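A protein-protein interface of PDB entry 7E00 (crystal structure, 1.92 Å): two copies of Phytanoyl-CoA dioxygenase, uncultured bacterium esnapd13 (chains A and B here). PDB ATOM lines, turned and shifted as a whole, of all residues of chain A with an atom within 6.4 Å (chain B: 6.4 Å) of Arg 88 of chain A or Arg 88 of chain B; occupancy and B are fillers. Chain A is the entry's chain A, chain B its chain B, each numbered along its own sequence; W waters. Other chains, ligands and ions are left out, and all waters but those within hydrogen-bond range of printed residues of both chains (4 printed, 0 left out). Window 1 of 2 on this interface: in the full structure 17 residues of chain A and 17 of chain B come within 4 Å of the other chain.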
ATOM      1  N   HIS A   6     -11.842 -26.320  18.148  1.00  0.00           N
ATOM      2  CA  HIS A   6     -11.801 -25.096  17.360  1.00  0.00           C
ATOM      3  C   HIS A   6     -13.094 -24.311  17.523  1.00  0.00           C
ATOM      4  O   HIS A   6     -14.213 -24.906  17.552  1.00  0.00           O
ATOM      5  CB  HIS A   6     -11.598 -25.418  15.877  1.00  0.00           C
ATOM      6  CG  HIS A   6     -10.264 -25.976  15.556  1.00  0.00           C
ATOM      7  ND1 HIS A   6      -9.996 -26.537  14.337  1.00  0.00           N
ATOM      8  CD2 HIS A   6      -9.175 -26.204  16.323  1.00  0.00           C
ATOM      9  CE1 HIS A   6      -8.775 -27.028  14.332  1.00  0.00           C
ATOM     10  NE2 HIS A   6      -8.242 -26.808  15.513  1.00  0.00           N
ATOM     11  N   LEU A  83      -6.749 -18.913  15.652  1.00  0.00           N
ATOM     12  CA  LEU A  83      -6.724 -18.099  14.455  1.00  0.00           C
ATOM     13  C   LEU A  83      -7.086 -18.838  13.208  1.00  0.00           C
ATOM     14  O   LEU A  83      -8.017 -18.464  12.487  1.00  0.00           O
ATOM     15  CB  LEU A  83      -5.340 -17.477  14.344  1.00  0.00           C
ATOM     16  CG  LEU A  83      -4.822 -16.583  15.473  1.00  0.00           C
ATOM     17  CD1 LEU A  83      -3.404 -16.098  15.156  1.00  0.00           C
ATOM     18  CD2 LEU A  83      -5.801 -15.391  15.578  1.00  0.00           C
ATOM     19  N   LEU A  84      -6.455 -19.962  12.969  1.00  0.00           N
ATOM     20  CA  LEU A  84      -6.633 -20.640  11.691  1.00  0.00           C
ATOM     21  C   LEU A  84      -8.038 -21.015  11.357  1.00  0.00           C
ATOM     22  O   LEU A  84      -8.489 -20.863  10.210  1.00  0.00           O
ATOM     23  CB  LEU A  84      -5.697 -21.890  11.668  1.00  0.00           C
ATOM     24  CG  LEU A  84      -5.687 -22.691  10.385  1.00  0.00           C
ATOM     25  CD1 LEU A  84      -5.178 -21.873   9.260  1.00  0.00           C
ATOM     26  CD2 LEU A  84      -4.703 -23.854  10.519  1.00  0.00           C
ATOM     27  N   PRO A  85      -8.789 -21.553  12.314  1.00  0.00           N
ATOM     28  CA  PRO A  85     -10.155 -21.932  11.968  1.00  0.00           C
ATOM     29  C   PRO A  85     -11.082 -20.763  11.560  1.00  0.00           C
ATOM     30  O   PRO A  85     -11.908 -20.887  10.699  1.00  0.00           O
ATOM     31  CB  PRO A  85     -10.669 -22.552  13.280  1.00  0.00           C
ATOM     32  CG  PRO A  85      -9.460 -22.993  13.980  1.00  0.00           C
ATOM     33  CD  PRO A  85      -8.434 -21.938  13.675  1.00  0.00           C
ATOM     34  N   ILE A  86     -10.897 -19.617  12.141  1.00  0.00           N
ATOM     35  CA  ILE A  86     -11.647 -18.454  11.749  1.00  0.00           C
ATOM     36  C   ILE A  86     -11.187 -17.976  10.373  1.00  0.00           C
ATOM     37  O   ILE A  86     -12.036 -17.638   9.568  1.00  0.00           O
ATOM     38  CB  ILE A  86     -11.572 -17.359  12.823  1.00  0.00           C
ATOM     39  CG1 ILE A  86     -12.269 -17.850  14.107  1.00  0.00           C
ATOM     40  CG2 ILE A  86     -12.098 -16.016  12.303  1.00  0.00           C
ATOM     41  CD1 ILE A  86     -12.026 -16.995  15.343  1.00  0.00           C
ATOM     42  N   ALA A  87      -9.853 -17.913  10.095  1.00  0.00           N
ATOM     43  CA  ALA A  87      -9.450 -17.568   8.776  1.00  0.00           C
ATOM     44  C   ALA A  87     -10.062 -18.472   7.685  1.00  0.00           C
ATOM     45  O   ALA A  87     -10.476 -17.997   6.619  1.00  0.00           O
ATOM     46  CB  ALA A  87      -7.931 -17.538   8.661  1.00  0.00           C
ATOM     47  N   ARG A  88     -10.002 -19.774   7.916  1.00  0.00           N
ATOM     48  CA  ARG A  88     -10.660 -20.719   7.005  1.00  0.00           C
ATOM     49  C   ARG A  88     -12.168 -20.474   6.790  1.00  0.00           C
ATOM     50  O   ARG A  88     -12.696 -20.604   5.667  1.00  0.00           O
ATOM     51  CB  ARG A  88     -10.465 -22.139   7.562  1.00  0.00           C
ATOM     52  CG  ARG A  88      -9.053 -22.714   7.519  1.00  0.00           C
ATOM     53  CD  ARG A  88      -9.039 -24.054   8.195  1.00  0.00           C
ATOM     54  NE  ARG A  88      -7.775 -24.800   8.032  1.00  0.00           N
ATOM     55  CZ  ARG A  88      -7.540 -25.977   8.588  1.00  0.00           C
ATOM     56  NH1 ARG A  88      -8.480 -26.576   9.341  1.00  0.00           N
ATOM     57  NH2 ARG A  88      -6.418 -26.646   8.319  1.00  0.00           N
ATOM     58  N   GLN A  89     -12.846 -20.183   7.877  1.00  0.00           N
ATOM     59  CA  GLN A  89     -14.259 -19.969   7.890  1.00  0.00           C
ATOM     60  C   GLN A  89     -14.594 -18.684   7.120  1.00  0.00           C
ATOM     61  O   GLN A  89     -15.431 -18.689   6.245  1.00  0.00           O
ATOM     62  CB  GLN A  89     -14.711 -19.834   9.307  1.00  0.00           C
ATOM     63  CG  GLN A  89     -16.123 -19.193   9.447  1.00  0.00           C
ATOM     64  CD  GLN A  89     -16.524 -19.017  10.901  1.00  0.00           C
ATOM     65  OE1 GLN A  89     -15.701 -18.714  11.763  1.00  0.00           O
ATOM     66  NE2 GLN A  89     -17.814 -19.233  11.200  1.00  0.00           N
ATOM     67  N   LEU A  90     -13.874 -17.618   7.385  1.00  0.00           N
ATOM     68  CA  LEU A  90     -14.143 -16.339   6.682  1.00  0.00           C
ATOM     69  C   LEU A  90     -13.792 -16.347   5.203  1.00  0.00           C
ATOM     70  O   LEU A  90     -14.501 -15.760   4.386  1.00  0.00           O
ATOM     71  CB  LEU A  90     -13.452 -15.183   7.401  1.00  0.00           C
ATOM     72  CG  LEU A  90     -14.082 -14.811   8.764  1.00  0.00           C
ATOM     73  CD1 LEU A  90     -13.314 -13.679   9.391  1.00  0.00           C
ATOM     74  CD2 LEU A  90     -15.570 -14.433   8.681  1.00  0.00           C
ATOM     75  N   LEU A  91     -12.692 -17.011   4.848  1.00  0.00           N
ATOM     76  CA  LEU A  91     -12.296 -17.102   3.483  1.00  0.00           C
ATOM     77  C   LEU A  91     -12.905 -18.263   2.747  1.00  0.00           C
ATOM     78  O   LEU A  91     -12.778 -18.334   1.545  1.00  0.00           O
ATOM     79  CB  LEU A  91     -10.778 -17.026   3.360  1.00  0.00           C
ATOM     80  CG  LEU A  91     -10.121 -15.790   4.009  1.00  0.00           C
ATOM     81  CD1 LEU A  91      -8.660 -15.787   3.698  1.00  0.00           C
ATOM     82  CD2 LEU A  91     -10.706 -14.485   3.465  1.00  0.00           C
ATOM     83  N   ARG A  92     -13.564 -19.162   3.486  1.00  0.00           N
ATOM     84  CA  ARG A  92     -14.220 -20.308   2.953  1.00  0.00           C
ATOM     85  C   ARG A  92     -13.261 -21.105   2.050  1.00  0.00           C
ATOM     86  O   ARG A  92     -13.610 -21.498   0.952  1.00  0.00           O
ATOM     87  CB  ARG A  92     -15.491 -19.863   2.197  1.00  0.00           C
ATOM     88  CG  ARG A  92     -16.514 -19.145   3.099  1.00  0.00           C
ATOM     89  CD  ARG A  92     -17.676 -18.503   2.329  1.00  0.00           C
ATOM     90  NE  ARG A  92     -18.427 -19.623   1.835  1.00  0.00           N
ATOM     91  CZ  ARG A  92     -19.527 -19.548   1.078  1.00  0.00           C
ATOM     92  NH1 ARG A  92     -20.018 -18.375   0.684  1.00  0.00           N
ATOM     93  NH2 ARG A  92     -20.128 -20.661   0.709  1.00  0.00           N
ATOM     94  N   ASP A  93     -12.093 -21.383   2.563  1.00  0.00           N
ATOM     95  CA  ASP A  93     -11.079 -22.155   1.858  1.00  0.00           C
ATOM     96  C   ASP A  93     -10.081 -22.590   2.860  1.00  0.00           C
ATOM     97  O   ASP A  93     -10.085 -22.116   4.035  1.00  0.00           O
ATOM     98  CB  ASP A  93     -10.463 -21.234   0.793  1.00  0.00           C
ATOM     99  CG  ASP A  93      -9.689 -21.968  -0.295  1.00  0.00           C
ATOM    100  OD1 ASP A  93      -9.594 -23.210  -0.289  1.00  0.00           O
ATOM    101  OD2 ASP A  93      -9.078 -21.266  -1.126  1.00  0.00           O
ATOM    102  N   ASP A  94      -9.153 -23.448   2.444  1.00  0.00           N
ATOM    103  CA  ASP A  94      -7.873 -23.547   3.109  1.00  0.00           C
ATOM    104  C   ASP A  94      -7.131 -22.217   2.880  1.00  0.00           C
ATOM    105  O   ASP A  94      -7.441 -21.480   1.949  1.00  0.00           O
ATOM    106  CB  ASP A  94      -6.993 -24.636   2.569  1.00  0.00           C
ATOM    107  CG  ASP A  94      -7.256 -25.995   3.229  1.00  0.00           C
ATOM    108  OD1 ASP A  94      -7.584 -26.103   4.461  1.00  0.00           O
ATOM    109  OD2 ASP A  94      -7.071 -26.981   2.458  1.00  0.00           O
ATOM    110  N   VAL A  95      -6.185 -21.916   3.754  1.00  0.00           N
ATOM    111  CA  VAL A  95      -5.501 -20.657   3.739  1.00  0.00           C
ATOM    112  C   VAL A  95      -4.046 -20.799   3.985  1.00  0.00           C
ATOM    113  O   VAL A  95      -3.595 -21.843   4.431  1.00  0.00           O
ATOM    114  CB  VAL A  95      -6.065 -19.699   4.830  1.00  0.00           C
ATOM    115  CG1 VAL A  95      -7.553 -19.463   4.595  1.00  0.00           C
ATOM    116  CG2 VAL A  95      -5.745 -20.231   6.230  1.00  0.00           C
ATOM    117  N   PRO A 259      -1.350 -25.373   2.076  1.00  0.00           N
ATOM    118  CA  PRO A 259      -2.390 -25.099   3.072  1.00  0.00           C
ATOM    119  C   PRO A 259      -1.942 -25.280   4.490  1.00  0.00           C
ATOM    120  O   PRO A 259      -1.314 -26.301   4.846  1.00  0.00           O
ATOM    121  CB  PRO A 259      -3.531 -26.109   2.745  1.00  0.00           C
ATOM    122  CG  PRO A 259      -3.112 -26.813   1.503  1.00  0.00           C
ATOM    123  CD  PRO A 259      -1.703 -26.445   1.105  1.00  0.00           C
ATOM    124  N   LEU A 260      -2.279 -24.321   5.346  1.00  0.00           N
ATOM    125  CA  LEU A 260      -1.915 -24.419   6.698  1.00  0.00           C
ATOM    126  C   LEU A 260      -2.821 -25.410   7.433  1.00  0.00           C
ATOM    127  O   LEU A 260      -3.997 -25.468   7.142  1.00  0.00           O
ATOM    128  CB  LEU A 260      -2.043 -23.077   7.436  1.00  0.00           C
ATOM    129  CG  LEU A 260      -1.000 -22.036   7.003  1.00  0.00           C
ATOM    130  CD1 LEU A 260      -1.355 -20.666   7.513  1.00  0.00           C
ATOM    131  CD2 LEU A 260       0.412 -22.418   7.451  1.00  0.00           C
ATOM    132  N   THR A 261      -2.220 -26.126   8.383  1.00  0.00           N
ATOM    133  CA  THR A 261      -2.912 -26.970   9.323  1.00  0.00           C
ATOM    134  C   THR A 261      -2.722 -26.517  10.751  1.00  0.00           C
ATOM    135  O   THR A 261      -1.778 -25.880  11.087  1.00  0.00           O
ATOM    136  CB  THR A 261      -2.428 -28.467   9.130  1.00  0.00           C
ATOM    137  OG1 THR A 261      -1.088 -28.571   9.467  1.00  0.00           O
ATOM    138  CG2 THR A 261      -2.512 -28.898   7.731  1.00  0.00           C
ATOM    139  N   ALA A 262      -3.644 -26.874  11.624  1.00  0.00           N
ATOM    140  CA  ALA A 262      -3.665 -26.351  12.953  1.00  0.00           C
ATOM    141  C   ALA A 262      -2.652 -27.043  13.861  1.00  0.00           C
ATOM    142  O   ALA A 262      -2.270 -28.190  13.667  1.00  0.00           O
ATOM    143  CB  ALA A 262      -5.015 -26.494  13.544  1.00  0.00           C
ATOM    144  N   HIS B   6     -16.159 -23.021   0.228  1.00  0.00           N
ATOM    145  CA  HIS B   6     -16.551 -24.083   1.191  1.00  0.00           C
ATOM    146  C   HIS B   6     -17.843 -23.708   1.851  1.00  0.00           C
ATOM    147  O   HIS B   6     -18.050 -22.523   2.249  1.00  0.00           O
ATOM    148  CB  HIS B   6     -15.461 -24.259   2.275  1.00  0.00           C
ATOM    149  CG  HIS B   6     -14.195 -24.810   1.738  1.00  0.00           C
ATOM    150  ND1 HIS B   6     -13.076 -24.995   2.505  1.00  0.00           N
ATOM    151  CD2 HIS B   6     -13.842 -25.143   0.475  1.00  0.00           C
ATOM    152  CE1 HIS B   6     -12.111 -25.490   1.769  1.00  0.00           C
ATOM    153  NE2 HIS B   6     -12.564 -25.623   0.540  1.00  0.00           N
ATOM    154  N   LEU B  83     -17.076 -32.213   1.410  1.00  0.00           N
ATOM    155  CA  LEU B  83     -17.055 -33.047   2.584  1.00  0.00           C
ATOM    156  C   LEU B  83     -16.151 -32.521   3.695  1.00  0.00           C
ATOM    157  O   LEU B  83     -16.527 -32.475   4.869  1.00  0.00           O
ATOM    158  CB  LEU B  83     -16.592 -34.451   2.191  1.00  0.00           C
ATOM    159  CG  LEU B  83     -17.558 -35.164   1.224  1.00  0.00           C
ATOM    160  CD1 LEU B  83     -16.921 -36.452   0.853  1.00  0.00           C
ATOM    161  CD2 LEU B  83     -18.942 -35.412   1.914  1.00  0.00           C
ATOM    162  N   LEU B  84     -14.912 -32.260   3.343  1.00  0.00           N
ATOM    163  CA  LEU B  84     -13.914 -31.910   4.346  1.00  0.00           C
ATOM    164  C   LEU B  84     -14.258 -30.746   5.208  1.00  0.00           C
ATOM    165  O   LEU B  84     -14.054 -30.839   6.441  1.00  0.00           O
ATOM    166  CB  LEU B  84     -12.521 -31.755   3.666  1.00  0.00           C
ATOM    167  CG  LEU B  84     -11.342 -31.521   4.610  1.00  0.00           C
ATOM    168  CD1 LEU B  84     -11.153 -32.648   5.530  1.00  0.00           C
ATOM    169  CD2 LEU B  84     -10.082 -31.288   3.801  1.00  0.00           C
ATOM    170  N   PRO B  85     -14.793 -29.646   4.667  1.00  0.00           N
ATOM    171  CA  PRO B  85     -15.082 -28.535   5.586  1.00  0.00           C
ATOM    172  C   PRO B  85     -16.115 -28.862   6.644  1.00  0.00           C
ATOM    173  O   PRO B  85     -16.029 -28.341   7.742  1.00  0.00           O
ATOM    174  CB  PRO B  85     -15.653 -27.442   4.688  1.00  0.00           C
ATOM    175  CG  PRO B  85     -15.124 -27.756   3.344  1.00  0.00           C
ATOM    176  CD  PRO B  85     -14.951 -29.247   3.267  1.00  0.00           C
ATOM    177  N   ILE B  86     -17.111 -29.690   6.316  1.00  0.00           N
ATOM    178  CA  ILE B  86     -18.112 -30.104   7.309  1.00  0.00           C
ATOM    179  C   ILE B  86     -17.594 -31.053   8.364  1.00  0.00           C
ATOM    180  O   ILE B  86     -17.851 -30.905   9.564  1.00  0.00           O
ATOM    181  CB  ILE B  86     -19.330 -30.697   6.557  1.00  0.00           C
ATOM    182  CG1 ILE B  86     -20.089 -29.466   5.923  1.00  0.00           C
ATOM    183  CG2 ILE B  86     -20.262 -31.437   7.536  1.00  0.00           C
ATOM    184  CD1 ILE B  86     -20.940 -29.877   4.792  1.00  0.00           C
ATOM    185  N   ALA B  87     -16.794 -32.019   7.930  1.00  0.00           N
ATOM    186  CA  ALA B  87     -16.110 -32.794   8.929  1.00  0.00           C
ATOM    187  C   ALA B  87     -15.248 -32.017   9.918  1.00  0.00           C
ATOM    188  O   ALA B  87     -15.345 -32.230  11.121  1.00  0.00           O
ATOM    189  CB  ALA B  87     -15.286 -33.832   8.258  1.00  0.00           C
ATOM    190  N   ARG B  88     -14.432 -31.089   9.408  1.00  0.00           N
ATOM    191  CA  ARG B  88     -13.696 -30.129  10.249  1.00  0.00           C
ATOM    192  C   ARG B  88     -14.600 -29.359  11.167  1.00  0.00           C
ATOM    193  O   ARG B  88     -14.267 -29.153  12.328  1.00  0.00           O
ATOM    194  CB  ARG B  88     -12.890 -29.103   9.382  1.00  0.00           C
ATOM    195  CG  ARG B  88     -11.669 -29.718   8.657  1.00  0.00           C
ATOM    196  CD  ARG B  88     -11.143 -28.678   7.677  1.00  0.00           C
ATOM    197  NE  ARG B  88      -9.877 -29.032   7.112  1.00  0.00           N
ATOM    198  CZ  ARG B  88      -9.227 -28.212   6.296  1.00  0.00           C
ATOM    199  NH1 ARG B  88      -9.755 -27.018   5.938  1.00  0.00           N
ATOM    200  NH2 ARG B  88      -8.077 -28.556   5.806  1.00  0.00           N
ATOM    201  N   GLN B  89     -15.732 -28.926  10.642  1.00  0.00           N
ATOM    202  CA  GLN B  89     -16.650 -28.115  11.375  1.00  0.00           C
ATOM    203  C   GLN B  89     -17.270 -28.958  12.515  1.00  0.00           C
ATOM    204  O   GLN B  89     -17.331 -28.515  13.650  1.00  0.00           O
ATOM    205  CB  GLN B  89     -17.764 -27.593  10.494  1.00  0.00           C
ATOM    206  CG  GLN B  89     -18.889 -26.863  11.208  1.00  0.00           C
ATOM    207  CD  GLN B  89     -20.050 -26.502  10.273  1.00  0.00           C
ATOM    208  OE1 GLN B  89     -20.264 -27.066   9.185  1.00  0.00           O
ATOM    209  NE2 GLN B  89     -20.797 -25.524  10.687  1.00  0.00           N
ATOM    210  N   LEU B  90     -17.696 -30.172  12.200  1.00  0.00           N
ATOM    211  CA  LEU B  90     -18.472 -30.927  13.170  1.00  0.00           C
ATOM    212  C   LEU B  90     -17.524 -31.502  14.237  1.00  0.00           C
ATOM    213  O   LEU B  90     -17.893 -31.590  15.407  1.00  0.00           O
ATOM    214  CB  LEU B  90     -19.257 -32.024  12.475  1.00  0.00           C
ATOM    215  CG  LEU B  90     -20.540 -31.589  11.715  1.00  0.00           C
ATOM    216  CD1 LEU B  90     -21.149 -32.750  11.060  1.00  0.00           C
ATOM    217  CD2 LEU B  90     -21.513 -30.950  12.673  1.00  0.00           C
ATOM    218  N   LEU B  91     -16.300 -31.907  13.847  1.00  0.00           N
ATOM    219  CA  LEU B  91     -15.339 -32.387  14.792  1.00  0.00           C
ATOM    220  C   LEU B  91     -14.481 -31.319  15.487  1.00  0.00           C
ATOM    221  O   LEU B  91     -13.732 -31.651  16.451  1.00  0.00           O
ATOM    222  CB  LEU B  91     -14.525 -33.499  14.202  1.00  0.00           C
ATOM    223  CG  LEU B  91     -15.314 -34.669  13.621  1.00  0.00           C
ATOM    224  CD1 LEU B  91     -14.302 -35.618  13.056  1.00  0.00           C
ATOM    225  CD2 LEU B  91     -16.136 -35.325  14.743  1.00  0.00           C
ATOM    226  N   ARG B  92     -14.631 -30.085  15.037  1.00  0.00           N
ATOM    227  CA  ARG B  92     -13.956 -28.905  15.529  1.00  0.00           C
ATOM    228  C   ARG B  92     -12.457 -29.125  15.639  1.00  0.00           C
ATOM    229  O   ARG B  92     -11.803 -28.804  16.671  1.00  0.00           O
ATOM    230  CB  ARG B  92     -14.555 -28.461  16.871  1.00  0.00           C
ATOM    231  CG  ARG B  92     -16.060 -28.138  16.786  1.00  0.00           C
ATOM    232  CD  ARG B  92     -16.693 -28.001  18.161  1.00  0.00           C
ATOM    233  NE  ARG B  92     -16.220 -26.727  18.740  1.00  0.00           N
ATOM    234  CZ  ARG B  92     -16.499 -26.266  19.968  1.00  0.00           C
ATOM    235  NH1 ARG B  92     -17.237 -26.969  20.822  1.00  0.00           N
ATOM    236  NH2 ARG B  92     -15.981 -25.111  20.367  1.00  0.00           N
ATOM    237  N   ASP B  93     -11.894 -29.649  14.566  1.00  0.00           N
ATOM    238  CA  ASP B  93     -10.489 -29.989  14.492  1.00  0.00           C
ATOM    239  C   ASP B  93     -10.110 -30.127  13.062  1.00  0.00           C
ATOM    240  O   ASP B  93     -10.970 -30.157  12.178  1.00  0.00           O
ATOM    241  CB  ASP B  93     -10.229 -31.337  15.181  1.00  0.00           C
ATOM    242  CG  ASP B  93      -8.804 -31.548  15.607  1.00  0.00           C
ATOM    243  OD1 ASP B  93      -7.870 -30.692  15.367  1.00  0.00           O
ATOM    244  OD2 ASP B  93      -8.555 -32.647  16.188  1.00  0.00           O
ATOM    245  N   ASP B  94      -8.821 -30.279  12.818  1.00  0.00           N
ATOM    246  CA  ASP B  94      -8.395 -30.900  11.583  1.00  0.00           C
ATOM    247  C   ASP B  94      -8.764 -32.369  11.651  1.00  0.00           C
ATOM    248  O   ASP B  94      -8.901 -32.938  12.729  1.00  0.00           O
ATOM    249  CB  ASP B  94      -6.878 -30.832  11.373  1.00  0.00           C
ATOM    250  CG  ASP B  94      -6.433 -29.535  10.640  1.00  0.00           C
ATOM    251  OD1 ASP B  94      -7.104 -29.036   9.667  1.00  0.00           O
ATOM    252  OD2 ASP B  94      -5.344 -29.059  11.049  1.00  0.00           O
ATOM    253  N   VAL B  95      -8.911 -32.994  10.498  1.00  0.00           N
ATOM    254  CA  VAL B  95      -9.311 -34.357  10.451  1.00  0.00           C
ATOM    255  C   VAL B  95      -8.503 -35.208   9.476  1.00  0.00           C
ATOM    256  O   VAL B  95      -7.761 -34.716   8.605  1.00  0.00           O
ATOM    257  CB  VAL B  95     -10.787 -34.478  10.032  1.00  0.00           C
ATOM    258  CG1 VAL B  95     -11.753 -33.703  11.002  1.00  0.00           C
ATOM    259  CG2 VAL B  95     -10.950 -33.952   8.639  1.00  0.00           C
ATOM    260  N   PRO B 259      -3.050 -34.238   8.736  1.00  0.00           N
ATOM    261  CA  PRO B 259      -4.310 -33.561   8.536  1.00  0.00           C
ATOM    262  C   PRO B 259      -4.636 -33.391   7.089  1.00  0.00           C
ATOM    263  O   PRO B 259      -3.772 -33.053   6.261  1.00  0.00           O
ATOM    264  CB  PRO B 259      -4.111 -32.177   9.248  1.00  0.00           C
ATOM    265  CG  PRO B 259      -2.835 -32.237   9.924  1.00  0.00           C
ATOM    266  CD  PRO B 259      -2.042 -33.405   9.463  1.00  0.00           C
ATOM    267  N   LEU B 260      -5.879 -33.704   6.736  1.00  0.00           N
ATOM    268  CA  LEU B 260      -6.285 -33.474   5.329  1.00  0.00           C
ATOM    269  C   LEU B 260      -6.481 -31.969   4.950  1.00  0.00           C
ATOM    270  O   LEU B 260      -6.905 -31.211   5.761  1.00  0.00           O
ATOM    271  CB  LEU B 260      -7.597 -34.199   5.048  1.00  0.00           C
ATOM    272  CG  LEU B 260      -7.531 -35.729   5.161  1.00  0.00           C
ATOM    273  CD1 LEU B 260      -8.920 -36.313   5.218  1.00  0.00           C
ATOM    274  CD2 LEU B 260      -6.709 -36.338   4.030  1.00  0.00           C
ATOM    275  N   THR B 261      -6.108 -31.631   3.698  1.00  0.00           N
ATOM    276  CA  THR B 261      -6.362 -30.336   3.065  1.00  0.00           C
ATOM    277  C   THR B 261      -7.314 -30.557   1.904  1.00  0.00           C
ATOM    278  O   THR B 261      -7.380 -31.646   1.283  1.00  0.00           O
ATOM    279  CB  THR B 261      -5.031 -29.756   2.567  1.00  0.00           C
ATOM    280  OG1 THR B 261      -4.504 -30.556   1.497  1.00  0.00           O
ATOM    281  CG2 THR B 261      -4.011 -29.806   3.634  1.00  0.00           C
ATOM    282  N   ALA B 262      -8.053 -29.536   1.597  1.00  0.00           N
ATOM    283  CA  ALA B 262      -9.039 -29.567   0.551  1.00  0.00           C
ATOM    284  C   ALA B 262      -8.491 -29.610  -0.824  1.00  0.00           C
ATOM    285  O   ALA B 262      -7.375 -29.100  -1.138  1.00  0.00           O
ATOM    286  CB  ALA B 262      -9.951 -28.390   0.698  1.00  0.00           C
HETATM  287  O   HOH W   1      -3.582 -30.270  12.771  1.00  0.00           O
HETATM  288  O   HOH W   2     -12.045 -26.986  12.550  1.00  0.00           O
HETATM  289  O   HOH W   3      -6.286 -26.854  -0.203  1.00  0.00           O
HETATM  290  O   HOH W   4     -12.930 -23.679   4.930  1.00  0.00           O
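The backbone NH (N) of His 6 of chain A sits at hydrogen-bond distance from the backbone carbonyl oxygen (O) of Arg 92 of chain B (2.9 Å). The guanidinium group (NH2) of Arg 88 of chain A lies within salt-bridge range of the side-chain carboxylate (OD1) of Asp 94 of chain B (2.8 Å). The guanidinium group (NE) of Arg 92 of chain A sits at hydrogen-bond distance from the backbone carbonyl oxygen (O) of His 6 of chain B, at 3.0 Å. OD1 of Asp 94 of chain A lies within salt-bridge range of NH1 of Arg 88 of chain B. The backbone NH (N) of Ala 262 of chain B sits at hydrogen-bond distance from the side-chain carboxylate (OD2) of Asp 94 of chain A (2.9 Å). N of Ala 262 of chain A is in hydrogen-bond range of OD2 of Asp 94 of chain B, 2.8 Å away.
The backbone carbonyl oxygen of Arg 88 of chain A is in hydrogen-bond range of the backbone NH of Asp 93 of chain A (3.3 Å). OD1 of Asp 94 of chain A lies within salt-bridge range of NE of Arg 88 of chain A, 3.8 Å away. The guanidinium group of Arg 88 of chain A sits at hydrogen-bond distance from the backbone carbonyl oxygen of Leu 260 of chain A (2.9 Å). O of Arg 88 of chain B lies within hydrogen-bond range of N of Asp 93 of chain B (3.3 Å). The side-chain carboxylate (OD1) of Asp 94 of chain B lies within salt-bridge range of the guanidinium group (NE) of Arg 88 of chain B (3.8 Å). The guanidinium group of Arg 88 of chain B is in hydrogen-bond range of the backbone carbonyl oxygen of Leu 260 of chain B, at 2.9 Å.
CE1 of His 6 of chain A touches CA of Asp 93 of chain B, 3.4 Å away. His 6 of chain A touches Asp 94 of chain B (CE1 to N, 3.6 Å). Arg 88 of chain A touches Arg 88 of chain B. His 6 of chain B touches Asp 93 of chain A. N of Asp 94 of chain A touches CE1 of His 6 of chain B, at 3.7 Å. CB of Thr 261 of chain B touches OD2 of Asp 94 of chain A, 3.4 Å away. CG of Pro 259 of chain A touches CB of Thr 261 of chain B (3.7 Å). Thr 261 of chain A touches Asp 94 of chain B (CB to OD2, 3.5 Å). CB of Thr 261 of chain A touches CG of Pro 259 of chain B, at 3.9 Å.
Arg 88 of chain A touches just these residues of chain B: Arg 88 and Asp 94. Of the printed residues of chain B, Arg 92 of chain A touches His 6 (3.0 Å). Printed residues of chain B within 4 Å of Thr 261 of chain A: Asp 94 (3.5 Å) and Pro 259 (3.9 Å). Leu 84 of chain B touches none of the printed residues of chain A. Arg 88 of chain B touches two residues of chain A. Of the printed residues of chain A, Pro 259 of chain B touches Thr 261 (3.9 Å). Printed residues of chain A within 4 Å of Thr 261 of chain B: Asp 94 (3.4 Å) and Pro 259 (3.7 Å). Printed residues of chain A within 4 Å of Ala 262 of chain B: Asp 94.
Of the 18 printed residues of chain B, 8 touch a printed residue of chain A. Hydrophobic or aromatic side chains of chain B within 4 Å of the printed part of chain A: His 6, Pro 259 and Ala 262. Of the 18 printed residues of chain A, 8 touch a printed residue of chain B. Among the printed residues, Asp or Glu carboxylates within 4 Å of a Lys or Arg side-chain nitrogen of the other chain: Arg 88 of chain A with Asp 94 of chain B (2.8 Å) and Asp 94 of chain A with Arg 88 of chain B (2.8 Å).
His 6 of chain A touches Arg 92 of chain B, and with the chains exchanged Arg 92 of chain A touches His 6 of chain B. Arg 88 of chain B touches its own counterpart, Arg 88 of chain A. Asp 94 of chain A touches Thr 261 of chain B, and with the chains exchanged Thr 261 of chain A touches Asp 94 of chain B. Pro 259 of chain A touches Thr 261 of chain B, and with the chains exchanged Thr 261 of chain A touches Pro 259 of chain B. Of the 15 pairs that touch across the chains among the printed residues, 15 have their exchanged pair printed and touching as well.
Water W1 bridges the backbone carbonyl oxygen of Ala 262 of chain A (2.6 Å) and the side-chain carboxylate of Asp 94 of chain B (2.7 Å). Water W3 bridges O of Ala 262 of chain B (2.7 Å) and OD2 of Asp 94 of chain A (2.8 Å). Water W2 lies within hydrogen-bond range of ND1 of His 6 of chain A (2.8 Å), O of Arg 88 of chain B (3.1 Å) and N of Asp 93 of chain B (3.3 Å). Water W4 lies within hydrogen-bond range of a ring nitrogen (ND1) of His 6 of chain B (2.8 Å), the backbone carbonyl oxygen (O) of Arg 88 of chain A (3.2 Å) and the backbone carbonyl oxygen (O) of Asp 93 of chain A (3.4 Å).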
